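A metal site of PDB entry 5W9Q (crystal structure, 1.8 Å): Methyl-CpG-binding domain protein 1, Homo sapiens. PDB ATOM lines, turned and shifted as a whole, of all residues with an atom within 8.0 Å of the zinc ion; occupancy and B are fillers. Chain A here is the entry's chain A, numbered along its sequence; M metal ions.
The side-chain sulfur of Cys 25 lies close to the backbone NH of Arg 45, at 3.2 Å.
N of Phe 27 lies close to SG of Cys 25 (3.8 Å).
O of Cys 25 is in hydrogen-bond range of SG of Cys 29 (3.4 Å).
The side-chain sulfur (SG) of Cys 44 sits close to the backbone NH (N) of Trp 46, at 3.4 Å.
The backbone NH (N) of Arg 24 sits close to the side-chain sulfur (SG) of Cys 22 (3.4 Å).
N of Gly 23 lies close to SG of Cys 28 (3.3 Å).
The side-chain carboxylate (OD1) of Asp 26 is in salt-bridge range of the guanidinium group (NE) of Arg 45.
Gly 23 touches the zinc ion.
Arg 45 touches the zinc ion.
Six residues have an atom within 4 Å of the zinc ion: Cys 22, Gly 23, Cys 25, Cys 28, Cys 44 and Arg 45.
Along chain A the residues within 4 Å of the zinc ion span positions 22 to 45.
The zinc ion is bound by the side-chain sulfur of Cys 25 (2.3 Å), the side-chain sulfur of Cys 44 (2.3 Å), the side-chain sulfur of Cys 22 (2.3 Å) and the side-chain sulfur of Cys 28 (2.3 Å).
The zinc ion has four donor atoms within binding distance.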
ATOM      1  N   ARG A  18     -15.600  34.428   9.405  1.00  0.00           N
ATOM      2  CA  ARG A  18     -15.050  33.670   8.256  1.00  0.00           C
ATOM      3  C   ARG A  18     -15.951  33.747   6.992  1.00  0.00           C
ATOM      4  O   ARG A  18     -17.155  33.655   7.081  1.00  0.00           O
ATOM      5  CB  ARG A  18     -14.843  32.213   8.653  1.00  0.00           C
ATOM      6  CG  ARG A  18     -13.724  31.548   7.869  1.00  0.00           C
ATOM      7  CD  ARG A  18     -13.964  30.047   7.712  1.00  0.00           C
ATOM      8  NE  ARG A  18     -12.904  29.391   6.927  1.00  0.00           N
ATOM      9  CZ  ARG A  18     -11.663  29.158   7.348  1.00  0.00           C
ATOM     10  NH1 ARG A  18     -10.804  28.553   6.529  1.00  0.00           N
ATOM     11  NH2 ARG A  18     -11.252  29.531   8.578  1.00  0.00           N
ATOM     12  N   MET A  20     -15.701  32.051   3.636  1.00  0.00           N
ATOM     13  CA  MET A  20     -15.959  30.924   2.765  1.00  0.00           C
ATOM     14  C   MET A  20     -15.816  29.612   3.514  1.00  0.00           C
ATOM     15  O   MET A  20     -15.132  29.538   4.585  1.00  0.00           O
ATOM     16  CB  MET A  20     -14.951  30.932   1.606  1.00  0.00           C
ATOM     17  N   ASP A  21     -16.419  28.556   2.951  1.00  0.00           N
ATOM     18  CA  ASP A  21     -16.279  27.215   3.469  1.00  0.00           C
ATOM     19  C   ASP A  21     -14.844  26.788   3.313  1.00  0.00           C
ATOM     20  O   ASP A  21     -14.230  27.104   2.302  1.00  0.00           O
ATOM     21  CB  ASP A  21     -17.177  26.210   2.711  1.00  0.00           C
ATOM     22  CG  ASP A  21     -18.656  26.350   3.034  1.00  0.00           C
ATOM     23  OD1 ASP A  21     -19.011  26.970   4.036  1.00  0.00           O
ATOM     24  OD2 ASP A  21     -19.498  25.797   2.281  1.00  0.00           O
ATOM     25  N   CYS A  22     -14.338  26.065   4.292  1.00  0.00           N
ATOM     26  CA  CYS A  22     -12.941  25.638   4.304  1.00  0.00           C
ATOM     27  C   CYS A  22     -12.701  24.552   3.268  1.00  0.00           C
ATOM     28  O   CYS A  22     -11.613  24.487   2.693  1.00  0.00           O
ATOM     29  CB  CYS A  22     -12.512  25.154   5.701  1.00  0.00           C
ATOM     30  SG  CYS A  22     -12.783  23.411   6.126  1.00  0.00           S
ATOM     31  N   GLY A  23     -13.732  23.717   3.016  1.00  0.00           N
ATOM     32  CA  GLY A  23     -13.660  22.695   1.923  1.00  0.00           C
ATOM     33  C   GLY A  23     -12.800  21.470   2.234  1.00  0.00           C
ATOM     34  O   GLY A  23     -12.565  20.702   1.362  1.00  0.00           O
ATOM     35  N   ARG A  24     -12.370  21.318   3.495  1.00  0.00           N
ATOM     36  CA  ARG A  24     -11.534  20.186   3.987  1.00  0.00           C
ATOM     37  C   ARG A  24     -12.019  19.450   5.266  1.00  0.00           C
ATOM     38  O   ARG A  24     -11.698  18.287   5.456  1.00  0.00           O
ATOM     39  CB  ARG A  24     -10.102  20.662   4.239  1.00  0.00           C
ATOM     40  CG  ARG A  24      -9.353  21.135   2.995  1.00  0.00           C
ATOM     41  CD  ARG A  24      -8.886  19.957   2.136  1.00  0.00           C
ATOM     42  NE  ARG A  24      -8.319  20.392   0.857  1.00  0.00           N
ATOM     43  CZ  ARG A  24      -8.094  19.588  -0.184  1.00  0.00           C
ATOM     44  NH1 ARG A  24      -7.574  20.088  -1.309  1.00  0.00           N
ATOM     45  NH2 ARG A  24      -8.393  18.281  -0.134  1.00  0.00           N
ATOM     46  N   CYS A  25     -12.809  20.105   6.123  1.00  0.00           N
ATOM     47  CA  CYS A  25     -13.315  19.547   7.336  1.00  0.00           C
ATOM     48  C   CYS A  25     -14.421  18.430   7.025  1.00  0.00           C
ATOM     49  O   CYS A  25     -14.938  18.253   5.868  1.00  0.00           O
ATOM     50  CB  CYS A  25     -13.881  20.694   8.229  1.00  0.00           C
ATOM     51  SG  CYS A  25     -15.521  21.359   7.658  1.00  0.00           S
ATOM     52  N   ASP A  26     -14.775  17.670   8.043  1.00  0.00           N
ATOM     53  CA  ASP A  26     -15.752  16.562   7.819  1.00  0.00           C
ATOM     54  C   ASP A  26     -17.153  17.118   7.261  1.00  0.00           C
ATOM     55  O   ASP A  26     -17.691  16.577   6.323  1.00  0.00           O
ATOM     56  CB  ASP A  26     -15.898  15.703   9.062  1.00  0.00           C
ATOM     57  CG  ASP A  26     -16.353  16.468  10.286  1.00  0.00           C
ATOM     58  OD1 ASP A  26     -16.359  17.714  10.364  1.00  0.00           O
ATOM     59  OD2 ASP A  26     -16.697  15.814  11.228  1.00  0.00           O
ATOM     60  N   PHE A  27     -17.625  18.225   7.819  1.00  0.00           N
ATOM     61  CA  PHE A  27     -18.880  18.835   7.400  1.00  0.00           C
ATOM     62  C   PHE A  27     -18.851  19.392   5.958  1.00  0.00           C
ATOM     63  O   PHE A  27     -19.844  19.264   5.185  1.00  0.00           O
ATOM     64  CB  PHE A  27     -19.325  19.904   8.432  1.00  0.00           C
ATOM     65  CG  PHE A  27     -19.618  19.359   9.855  1.00  0.00           C
ATOM     66  CD1 PHE A  27     -20.031  18.066  10.078  1.00  0.00           C
ATOM     67  CD2 PHE A  27     -19.473  20.197  10.976  1.00  0.00           C
ATOM     68  CE1 PHE A  27     -20.317  17.621  11.350  1.00  0.00           C
ATOM     69  CE2 PHE A  27     -19.779  19.756  12.262  1.00  0.00           C
ATOM     70  CZ  PHE A  27     -20.179  18.457  12.447  1.00  0.00           C
ATOM     71  N   CYS A  28     -17.705  19.989   5.559  1.00  0.00           N
ATOM     72  CA  CYS A  28     -17.559  20.505   4.196  1.00  0.00           C
ATOM     73  C   CYS A  28     -17.526  19.371   3.213  1.00  0.00           C
ATOM     74  O   CYS A  28     -18.342  19.349   2.261  1.00  0.00           O
ATOM     75  CB  CYS A  28     -16.282  21.397   4.022  1.00  0.00           C
ATOM     76  SG  CYS A  28     -16.543  23.064   4.611  1.00  0.00           S
ATOM     77  N   CYS A  29     -16.583  18.447   3.422  1.00  0.00           N
ATOM     78  CA  CYS A  29     -16.504  17.211   2.587  1.00  0.00           C
ATOM     79  C   CYS A  29     -17.829  16.481   2.410  1.00  0.00           C
ATOM     80  O   CYS A  29     -18.044  15.866   1.392  1.00  0.00           O
ATOM     81  CB  CYS A  29     -15.505  16.236   3.187  1.00  0.00           C
ATOM     82  SG  CYS A  29     -13.875  16.913   2.943  1.00  0.00           S
ATOM     83  N   LYS A  31     -20.793  18.023   2.222  1.00  0.00           N
ATOM     84  CA  LYS A  31     -21.654  18.835   1.354  1.00  0.00           C
ATOM     85  C   LYS A  31     -21.660  18.299  -0.064  1.00  0.00           C
ATOM     86  O   LYS A  31     -20.613  17.979  -0.594  1.00  0.00           O
ATOM     87  CB  LYS A  31     -21.245  20.325   1.378  1.00  0.00           C
ATOM     88  CG  LYS A  31     -21.407  20.971   2.753  1.00  0.00           C
ATOM     89  CD  LYS A  31     -20.947  22.445   2.776  1.00  0.00           C
ATOM     90  CE  LYS A  31     -21.458  23.238   3.976  1.00  0.00           C
ATOM     91  NZ  LYS A  31     -22.964  23.297   3.842  1.00  0.00           N
ATOM     92  N   PHE A  34     -19.201  19.821  -2.510  1.00  0.00           N
ATOM     93  CA  PHE A  34     -17.807  19.343  -2.362  1.00  0.00           C
ATOM     94  C   PHE A  34     -17.632  17.874  -2.690  1.00  0.00           C
ATOM     95  O   PHE A  34     -16.496  17.358  -2.701  1.00  0.00           O
ATOM     96  CB  PHE A  34     -17.292  19.686  -0.975  1.00  0.00           C
ATOM     97  CG  PHE A  34     -17.004  21.153  -0.796  1.00  0.00           C
ATOM     98  CD1 PHE A  34     -16.158  21.825  -1.674  1.00  0.00           C
ATOM     99  CD2 PHE A  34     -17.550  21.866   0.265  1.00  0.00           C
ATOM    100  CE1 PHE A  34     -15.886  23.165  -1.493  1.00  0.00           C
ATOM    101  CE2 PHE A  34     -17.257  23.211   0.452  1.00  0.00           C
ATOM    102  CZ  PHE A  34     -16.448  23.866  -0.436  1.00  0.00           C
ATOM    103  N   GLN A  42     -24.241  19.829   8.207  1.00  0.00           N
ATOM    104  CA  GLN A  42     -23.843  20.861   9.141  1.00  0.00           C
ATOM    105  C   GLN A  42     -22.939  21.845   8.397  1.00  0.00           C
ATOM    106  O   GLN A  42     -22.314  21.537   7.345  1.00  0.00           O
ATOM    107  CB  GLN A  42     -23.086  20.243  10.297  1.00  0.00           C
ATOM    108  CG  GLN A  42     -23.846  19.130  11.078  1.00  0.00           C
ATOM    109  CD  GLN A  42     -25.179  19.547  11.677  1.00  0.00           C
ATOM    110  OE1 GLN A  42     -25.454  20.724  11.864  1.00  0.00           O
ATOM    111  NE2 GLN A  42     -26.050  18.515  11.980  1.00  0.00           N
ATOM    112  N   LYS A  43     -22.861  23.049   8.938  1.00  0.00           N
ATOM    113  CA  LYS A  43     -21.952  24.004   8.339  1.00  0.00           C
ATOM    114  C   LYS A  43     -20.505  23.700   8.671  1.00  0.00           C
ATOM    115  O   LYS A  43     -20.223  22.965   9.595  1.00  0.00           O
ATOM    116  CB  LYS A  43     -22.333  25.431   8.634  1.00  0.00           C
ATOM    117  CG  LYS A  43     -22.413  25.871  10.025  1.00  0.00           C
ATOM    118  CD  LYS A  43     -22.408  27.432  10.038  1.00  0.00           C
ATOM    119  CE  LYS A  43     -23.100  27.966  11.225  1.00  0.00           C
ATOM    120  NZ  LYS A  43     -22.964  29.442  11.243  1.00  0.00           N
ATOM    121  N   CYS A  44     -19.614  24.283   7.844  1.00  0.00           N
ATOM    122  CA  CYS A  44     -18.155  24.103   7.980  1.00  0.00           C
ATOM    123  C   CYS A  44     -17.780  24.124   9.453  1.00  0.00           C
ATOM    124  O   CYS A  44     -18.221  25.057  10.197  1.00  0.00           O
ATOM    125  CB  CYS A  44     -17.468  25.310   7.309  1.00  0.00           C
ATOM    126  SG  CYS A  44     -15.718  25.156   7.382  1.00  0.00           S
ATOM    127  N   ARG A  45     -16.989  23.166   9.881  1.00  0.00           N
ATOM    128  CA  ARG A  45     -16.477  23.180  11.286  1.00  0.00           C
ATOM    129  C   ARG A  45     -15.902  24.553  11.727  1.00  0.00           C
ATOM    130  O   ARG A  45     -16.107  25.020  12.889  1.00  0.00           O
ATOM    131  CB  ARG A  45     -15.346  22.198  11.439  1.00  0.00           C
ATOM    132  CG  ARG A  45     -15.734  20.761  11.479  1.00  0.00           C
ATOM    133  CD  ARG A  45     -16.366  20.392  12.812  1.00  0.00           C
ATOM    134  NE  ARG A  45     -16.674  18.961  12.825  1.00  0.00           N
ATOM    135  CZ  ARG A  45     -17.184  18.284  13.840  1.00  0.00           C
ATOM    136  NH1 ARG A  45     -17.522  18.872  14.992  1.00  0.00           N
ATOM    137  NH2 ARG A  45     -17.390  16.971  13.678  1.00  0.00           N
ATOM    138  N   TRP A  46     -15.191  25.183  10.788  1.00  0.00           N
ATOM    139  CA  TRP A  46     -14.469  26.493  11.033  1.00  0.00           C
ATOM    140  C   TRP A  46     -15.406  27.736  10.938  1.00  0.00           C
ATOM    141  O   TRP A  46     -14.960  28.862  11.212  1.00  0.00           O
ATOM    142  CB  TRP A  46     -13.291  26.621  10.074  1.00  0.00           C
ATOM    143  CG  TRP A  46     -12.386  25.526  10.306  1.00  0.00           C
ATOM    144  CD1 TRP A  46     -12.152  24.441   9.513  1.00  0.00           C
ATOM    145  CD2 TRP A  46     -11.621  25.333  11.486  1.00  0.00           C
ATOM    146  NE1 TRP A  46     -11.321  23.574  10.134  1.00  0.00           N
ATOM    147  CE2 TRP A  46     -10.966  24.085  11.355  1.00  0.00           C
ATOM    148  CE3 TRP A  46     -11.439  26.091  12.664  1.00  0.00           C
ATOM    149  CZ2 TRP A  46     -10.065  23.595  12.350  1.00  0.00           C
ATOM    150  CZ3 TRP A  46     -10.511  25.597  13.669  1.00  0.00           C
ATOM    151  CH2 TRP A  46      -9.871  24.362  13.498  1.00  0.00           C
ATOM    152  N   ARG A  47     -16.707  27.518  10.585  1.00  0.00           N
ATOM    153  CA  ARG A  47     -17.739  28.531  10.632  1.00  0.00           C
ATOM    154  C   ARG A  47     -18.768  28.305  11.731  1.00  0.00           C
ATOM    155  O   ARG A  47     -19.767  29.006  11.804  1.00  0.00           O
ATOM    156  CB  ARG A  47     -18.392  28.636   9.257  1.00  0.00           C
ATOM    157  CG  ARG A  47     -17.388  28.811   8.104  1.00  0.00           C
ATOM    158  CD  ARG A  47     -18.062  28.862   6.730  1.00  0.00           C
ATOM    159  NE  ARG A  47     -18.528  30.190   6.433  1.00  0.00           N
ATOM    160  CZ  ARG A  47     -19.134  30.577   5.300  1.00  0.00           C
ATOM    161  NH1 ARG A  47     -19.453  31.879   5.133  1.00  0.00           N
ATOM    162  NH2 ARG A  47     -19.380  29.726   4.327  1.00  0.00           N
HETATM  163 ZN    ZN M   1     -15.064  23.202   6.406  1.00  0.00          ZN
